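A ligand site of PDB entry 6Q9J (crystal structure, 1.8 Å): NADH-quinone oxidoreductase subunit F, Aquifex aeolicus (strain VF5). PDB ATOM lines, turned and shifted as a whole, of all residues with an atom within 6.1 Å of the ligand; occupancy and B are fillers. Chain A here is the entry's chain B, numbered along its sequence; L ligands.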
ATOM      1  N   ILE A 181      -6.151 -27.734   7.471  1.00  0.00           N
ATOM      2  CA  ILE A 181      -6.981 -26.862   8.341  1.00  0.00           C
ATOM      3  C   ILE A 181      -8.450 -26.967   7.935  1.00  0.00           C
ATOM      4  O   ILE A 181      -9.309 -26.687   8.774  1.00  0.00           O
ATOM      5  CB  ILE A 181      -6.461 -25.400   8.350  1.00  0.00           C
ATOM      6  CG1 ILE A 181      -7.118 -24.580   9.462  1.00  0.00           C
ATOM      7  CG2 ILE A 181      -6.619 -24.737   6.991  1.00  0.00           C
ATOM      8  CD1 ILE A 181      -7.073 -25.222  10.817  1.00  0.00           C
ATOM      9  N   HIS A 198     -10.336 -20.644   6.662  1.00  0.00           N
ATOM     10  CA  HIS A 198      -9.987 -19.907   7.904  1.00  0.00           C
ATOM     11  C   HIS A 198     -10.989 -20.279   8.999  1.00  0.00           C
ATOM     12  O   HIS A 198     -12.171 -19.957   8.890  1.00  0.00           O
ATOM     13  CB  HIS A 198      -9.960 -18.399   7.669  1.00  0.00           C
ATOM     14  CG  HIS A 198      -8.796 -17.933   6.852  1.00  0.00           C
ATOM     15  ND1 HIS A 198      -8.759 -16.689   6.275  1.00  0.00           N
ATOM     16  CD2 HIS A 198      -7.629 -18.531   6.529  1.00  0.00           C
ATOM     17  CE1 HIS A 198      -7.616 -16.538   5.629  1.00  0.00           C
ATOM     18  NE2 HIS A 198      -6.907 -17.650   5.765  1.00  0.00           N
ATOM     19  N   PRO A 199     -10.564 -20.980  10.074  1.00  0.00           N
ATOM     20  CA  PRO A 199     -11.431 -21.226  11.227  1.00  0.00           C
ATOM     21  C   PRO A 199     -12.090 -19.943  11.745  1.00  0.00           C
ATOM     22  O   PRO A 199     -11.509 -18.882  11.645  1.00  0.00           O
ATOM     23  CB  PRO A 199     -10.487 -21.818  12.271  1.00  0.00           C
ATOM     24  CG  PRO A 199      -9.400 -22.485  11.455  1.00  0.00           C
ATOM     25  CD  PRO A 199      -9.235 -21.591  10.243  1.00  0.00           C
ATOM     26  N   GLU A 345       0.889 -26.128   7.722  1.00  0.00           N
ATOM     27  CA  GLU A 345      -0.597 -26.186   7.772  1.00  0.00           C
ATOM     28  C   GLU A 345      -1.249 -25.009   8.527  1.00  0.00           C
ATOM     29  O   GLU A 345      -2.461 -24.819   8.321  1.00  0.00           O
ATOM     30  CB  GLU A 345      -1.063 -27.537   8.328  1.00  0.00           C
ATOM     31  CG  GLU A 345      -0.635 -28.733   7.488  1.00  0.00           C
ATOM     32  CD  GLU A 345      -1.043 -28.739   6.016  1.00  0.00           C
ATOM     33  OE1 GLU A 345      -1.975 -28.004   5.624  1.00  0.00           O
ATOM     34  OE2 GLU A 345      -0.401 -29.500   5.250  1.00  0.00           O
ATOM     35  N   THR A 346      -0.530 -24.261   9.359  1.00  0.00           N
ATOM     36  CA  THR A 346      -1.129 -23.070  10.045  1.00  0.00           C
ATOM     37  C   THR A 346      -1.723 -22.143   8.981  1.00  0.00           C
ATOM     38  O   THR A 346      -1.058 -21.912   7.965  1.00  0.00           O
ATOM     39  CB  THR A 346      -0.118 -22.331  10.945  1.00  0.00           C
ATOM     40  OG1 THR A 346      -0.802 -21.173  11.420  1.00  0.00           O
ATOM     41  CG2 THR A 346       1.153 -21.932  10.236  1.00  0.00           C
ATOM     42  N   CYS A 347      -2.945 -21.641   9.196  1.00  0.00           N
ATOM     43  CA  CYS A 347      -3.637 -20.737   8.240  1.00  0.00           C
ATOM     44  C   CYS A 347      -3.144 -19.293   8.427  1.00  0.00           C
ATOM     45  O   CYS A 347      -3.376 -18.468   7.537  1.00  0.00           O
ATOM     46  CB  CYS A 347      -5.152 -20.846   8.371  1.00  0.00           C
ATOM     47  SG  CYS A 347      -5.860 -19.961   9.789  1.00  0.00           S
ATOM     48  N   GLY A 348      -2.499 -18.981   9.569  1.00  0.00           N
ATOM     49  CA  GLY A 348      -1.821 -17.694   9.799  1.00  0.00           C
ATOM     50  C   GLY A 348      -2.697 -16.576  10.349  1.00  0.00           C
ATOM     51  O   GLY A 348      -2.180 -15.466  10.508  1.00  0.00           O
ATOM     52  N   GLN A 349      -3.969 -16.836  10.672  1.00  0.00           N
ATOM     53  CA  GLN A 349      -4.901 -15.804  11.218  1.00  0.00           C
ATOM     54  C   GLN A 349      -4.404 -15.276  12.561  1.00  0.00           C
ATOM     55  O   GLN A 349      -4.548 -14.051  12.809  1.00  0.00           O
ATOM     56  CB  GLN A 349      -6.295 -16.380  11.493  1.00  0.00           C
ATOM     57  CG  GLN A 349      -7.209 -16.443  10.278  1.00  0.00           C
ATOM     58  CD  GLN A 349      -8.597 -16.788  10.760  1.00  0.00           C
ATOM     59  OE1 GLN A 349      -9.428 -15.898  10.939  1.00  0.00           O
ATOM     60  NE2 GLN A 349      -8.828 -18.062  11.039  1.00  0.00           N
ATOM     61  N   CYS A 350      -3.918 -16.170  13.418  1.00  0.00           N
ATOM     62  CA  CYS A 350      -3.492 -15.893  14.815  1.00  0.00           C
ATOM     63  C   CYS A 350      -1.964 -15.750  14.847  1.00  0.00           C
ATOM     64  O   CYS A 350      -1.292 -16.639  14.320  1.00  0.00           O
ATOM     65  CB  CYS A 350      -3.940 -16.997  15.769  1.00  0.00           C
ATOM     66  SG  CYS A 350      -5.629 -17.555  15.470  1.00  0.00           S
ATOM     67  N   THR A 351      -1.452 -14.686  15.444  1.00  0.00           N
ATOM     68  CA  THR A 351      -0.018 -14.307  15.341  1.00  0.00           C
ATOM     69  C   THR A 351       0.854 -15.381  15.985  1.00  0.00           C
ATOM     70  O   THR A 351       1.789 -15.847  15.346  1.00  0.00           O
ATOM     71  CB  THR A 351       0.217 -12.884  15.847  1.00  0.00           C
ATOM     72  OG1 THR A 351      -0.322 -12.002  14.862  1.00  0.00           O
ATOM     73  CG2 THR A 351       1.687 -12.591  16.082  1.00  0.00           C
ATOM     74  N   CYS A 353       0.376 -18.546  16.554  1.00  0.00           N
ATOM     75  CA  CYS A 353       0.294 -19.765  15.695  1.00  0.00           C
ATOM     76  C   CYS A 353       1.103 -19.539  14.412  1.00  0.00           C
ATOM     77  O   CYS A 353       1.972 -20.380  14.092  1.00  0.00           O
ATOM     78  CB  CYS A 353      -1.148 -20.125  15.355  1.00  0.00           C
ATOM     79  SG  CYS A 353      -1.299 -21.687  14.457  1.00  0.00           S
ATOM     80  N   ARG A 354       0.849 -18.439  13.698  1.00  0.00           N
ATOM     81  CA  ARG A 354       1.543 -18.103  12.423  1.00  0.00           C
ATOM     82  C   ARG A 354       3.062 -18.136  12.637  1.00  0.00           C
ATOM     83  O   ARG A 354       3.746 -18.892  11.913  1.00  0.00           O
ATOM     84  CB  ARG A 354       1.089 -16.729  11.914  1.00  0.00           C
ATOM     85  CG  ARG A 354       1.754 -16.305  10.613  1.00  0.00           C
ATOM     86  CD  ARG A 354       1.209 -14.976  10.098  1.00  0.00           C
ATOM     87  NE  ARG A 354       1.556 -13.855  10.974  1.00  0.00           N
ATOM     88  CZ  ARG A 354       0.716 -13.217  11.792  1.00  0.00           C
ATOM     89  NH1 ARG A 354      -0.568 -13.559  11.863  1.00  0.00           N
ATOM     90  NH2 ARG A 354       1.178 -12.207  12.526  1.00  0.00           N
ATOM     91  N   CYS A 357       4.507 -21.748  14.714  1.00  0.00           N
ATOM     92  CA  CYS A 357       4.605 -22.998  13.904  1.00  0.00           C
ATOM     93  C   CYS A 357       5.830 -22.888  12.982  1.00  0.00           C
ATOM     94  O   CYS A 357       6.572 -23.880  12.882  1.00  0.00           O
ATOM     95  CB  CYS A 357       3.348 -23.264  13.090  1.00  0.00           C
ATOM     96  SG  CYS A 357       1.964 -23.793  14.139  1.00  0.00           S
ATOM     97  N   THR A 390      -3.887 -16.879  22.212  1.00  0.00           N
ATOM     98  CA  THR A 390      -4.847 -16.159  21.326  1.00  0.00           C
ATOM     99  C   THR A 390      -5.398 -17.068  20.211  1.00  0.00           C
ATOM    100  O   THR A 390      -6.256 -16.567  19.466  1.00  0.00           O
ATOM    101  CB  THR A 390      -4.253 -14.881  20.728  1.00  0.00           C
ATOM    102  OG1 THR A 390      -3.415 -15.222  19.617  1.00  0.00           O
ATOM    103  CG2 THR A 390      -3.482 -14.064  21.736  1.00  0.00           C
ATOM    104  N   SER A 391      -4.969 -18.331  20.118  1.00  0.00           N
ATOM    105  CA  SER A 391      -5.389 -19.264  19.031  1.00  0.00           C
ATOM    106  C   SER A 391      -6.910 -19.444  19.047  1.00  0.00           C
ATOM    107  O   SER A 391      -7.497 -19.497  20.156  1.00  0.00           O
ATOM    108  CB  SER A 391      -4.675 -20.590  19.151  1.00  0.00           C
ATOM    109  OG  SER A 391      -5.013 -21.250  20.354  1.00  0.00           O
ATOM    110  N   ILE A 392      -7.550 -19.514  17.876  1.00  0.00           N
ATOM    111  CA  ILE A 392      -9.022 -19.664  17.762  1.00  0.00           C
ATOM    112  C   ILE A 392      -9.375 -21.049  17.192  1.00  0.00           C
ATOM    113  O   ILE A 392     -10.564 -21.258  16.898  1.00  0.00           O
ATOM    114  CB  ILE A 392      -9.669 -18.513  16.963  1.00  0.00           C
ATOM    115  CG1 ILE A 392      -9.242 -18.490  15.492  1.00  0.00           C
ATOM    116  CG2 ILE A 392      -9.393 -17.175  17.644  1.00  0.00           C
ATOM    117  CD1 ILE A 392     -10.029 -17.511  14.648  1.00  0.00           C
ATOM    118  N   CYS A 393      -8.409 -21.970  17.060  1.00  0.00           N
ATOM    119  CA  CYS A 393      -8.720 -23.381  16.703  1.00  0.00           C
ATOM    120  C   CYS A 393      -7.674 -24.334  17.300  1.00  0.00           C
ATOM    121  O   CYS A 393      -6.665 -23.862  17.854  1.00  0.00           O
ATOM    122  CB  CYS A 393      -8.875 -23.568  15.194  1.00  0.00           C
ATOM    123  SG  CYS A 393      -7.360 -24.065  14.324  1.00  0.00           S
ATOM    124  N   GLY A 394      -7.956 -25.628  17.203  1.00  0.00           N
ATOM    125  CA  GLY A 394      -7.193 -26.716  17.841  1.00  0.00           C
ATOM    126  C   GLY A 394      -5.773 -26.822  17.330  1.00  0.00           C
ATOM    127  O   GLY A 394      -4.966 -27.401  18.074  1.00  0.00           O
ATOM    128  N   LEU A 395      -5.457 -26.334  16.131  1.00  0.00           N
ATOM    129  CA  LEU A 395      -4.101 -26.465  15.519  1.00  0.00           C
ATOM    130  C   LEU A 395      -3.095 -25.696  16.401  1.00  0.00           C
ATOM    131  O   LEU A 395      -2.141 -26.332  16.903  1.00  0.00           O
ATOM    132  CB  LEU A 395      -4.119 -25.951  14.081  1.00  0.00           C
ATOM    133  CG  LEU A 395      -2.898 -26.309  13.222  1.00  0.00           C
ATOM    134  CD1 LEU A 395      -3.248 -26.333  11.751  1.00  0.00           C
ATOM    135  CD2 LEU A 395      -1.734 -25.351  13.471  1.00  0.00           C
ATOM    136  N   GLY A 396      -3.305 -24.394  16.602  1.00  0.00           N
ATOM    137  CA  GLY A 396      -2.474 -23.566  17.491  1.00  0.00           C
ATOM    138  C   GLY A 396      -2.446 -24.112  18.907  1.00  0.00           C
ATOM    139  O   GLY A 396      -1.387 -24.040  19.556  1.00  0.00           O
ATOM    140  N   ALA A 397      -3.558 -24.677  19.373  1.00  0.00           N
ATOM    141  CA  ALA A 397      -3.698 -25.256  20.735  1.00  0.00           C
ATOM    142  C   ALA A 397      -2.744 -26.445  20.939  1.00  0.00           C
ATOM    143  O   ALA A 397      -2.345 -26.666  22.100  1.00  0.00           O
ATOM    144  CB  ALA A 397      -5.123 -25.648  21.015  1.00  0.00           C
HETATM  145 FE1  LIG L   1      -5.246 -20.610  11.876  1.00  0.00          FE
HETATM  146 FE2  LIG L   1      -3.488 -21.433  13.814  1.00  0.00          FE
HETATM  147 FE3  LIG L   1      -6.092 -22.195  13.928  1.00  0.00          FE
HETATM  148 FE4  LIG L   1      -5.370 -19.566  14.393  1.00  0.00          FE
HETATM  149  S1  LIG L   1      -4.794 -21.407  15.656  1.00  0.00           S
HETATM  150  S2  LIG L   1      -7.135 -20.296  13.122  1.00  0.00           S
HETATM  151  S3  LIG L   1      -3.664 -19.325  12.906  1.00  0.00           S
HETATM  152  S4  LIG L   1      -4.583 -22.747  12.305  1.00  0.00           S
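NE2 of Gln 349 lies close to SG of Cys 347, 3.7 Å away. The side-chain sulfur (SG) of Cys 393 lies close to the backbone NH (N) of Leu 395, at 3.5 Å. SG of Cys 353 lies close to OG1 of Thr 346 (3.1 Å). SG of Cys 357 lies close to O of Cys 353 (3.4 Å). The side-chain sulfur (SG) of Cys 350 sits close to the backbone NH (N) of Ile 392. The backbone carbonyl oxygen (O) of Pro 199 is in hydrogen-bond range of the side-chain amide nitrogen (NE2) of Gln 349. N of Gly 348 lies close to OG1 of Thr 346, 3.3 Å away. The backbone carbonyl oxygen of Gly 348 lies within hydrogen-bond range of the guanidinium group of Arg 354, at 2.8 Å.
Residues that only touch the ligand: Ile 181, Pro 199, Ser 391, Ile 392 and Leu 395. Hydrophobic or aromatic side chains within 4 Å of the ligand: Ile 181, Pro 199, Ile 392 and Leu 395. Of the 21 residues printed, 13 come within 4 Å of the ligand.
A sulfur (S4) of the ligand lies close to the backbone NH (N) of Cys 347. The side-chain sulfur of Cys 347 is bound to an iron atom (FE1) of the ligand, at 2.3 Å. The side-chain sulfur of Cys 393 is bound to an iron atom (FE3) of the ligand (2.3 Å). FE2 of the ligand is bound by SG of Cys 353, 2.3 Å away. The backbone NH (N) of Cys 350 sits close to a sulfur (S3) of the ligand (3.2 Å). The side-chain sulfur of Cys 350 is bound to an iron atom (FE4) of the ligand (2.3 Å). N of Gln 349 sits close to S3 of the ligand (3.4 Å). S2 of the ligand lies close to NE2 of Gln 349 (3.5 Å). A sulfur (S1) of the ligand sits close to the backbone NH (N) of Gly 396 (3.5 Å). The backbone NH of Gly 348 lies close to a sulfur (S3) of the ligand (3.6 Å). S3 of the ligand lies close to OG1 of Thr 346 (3.7 Å).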
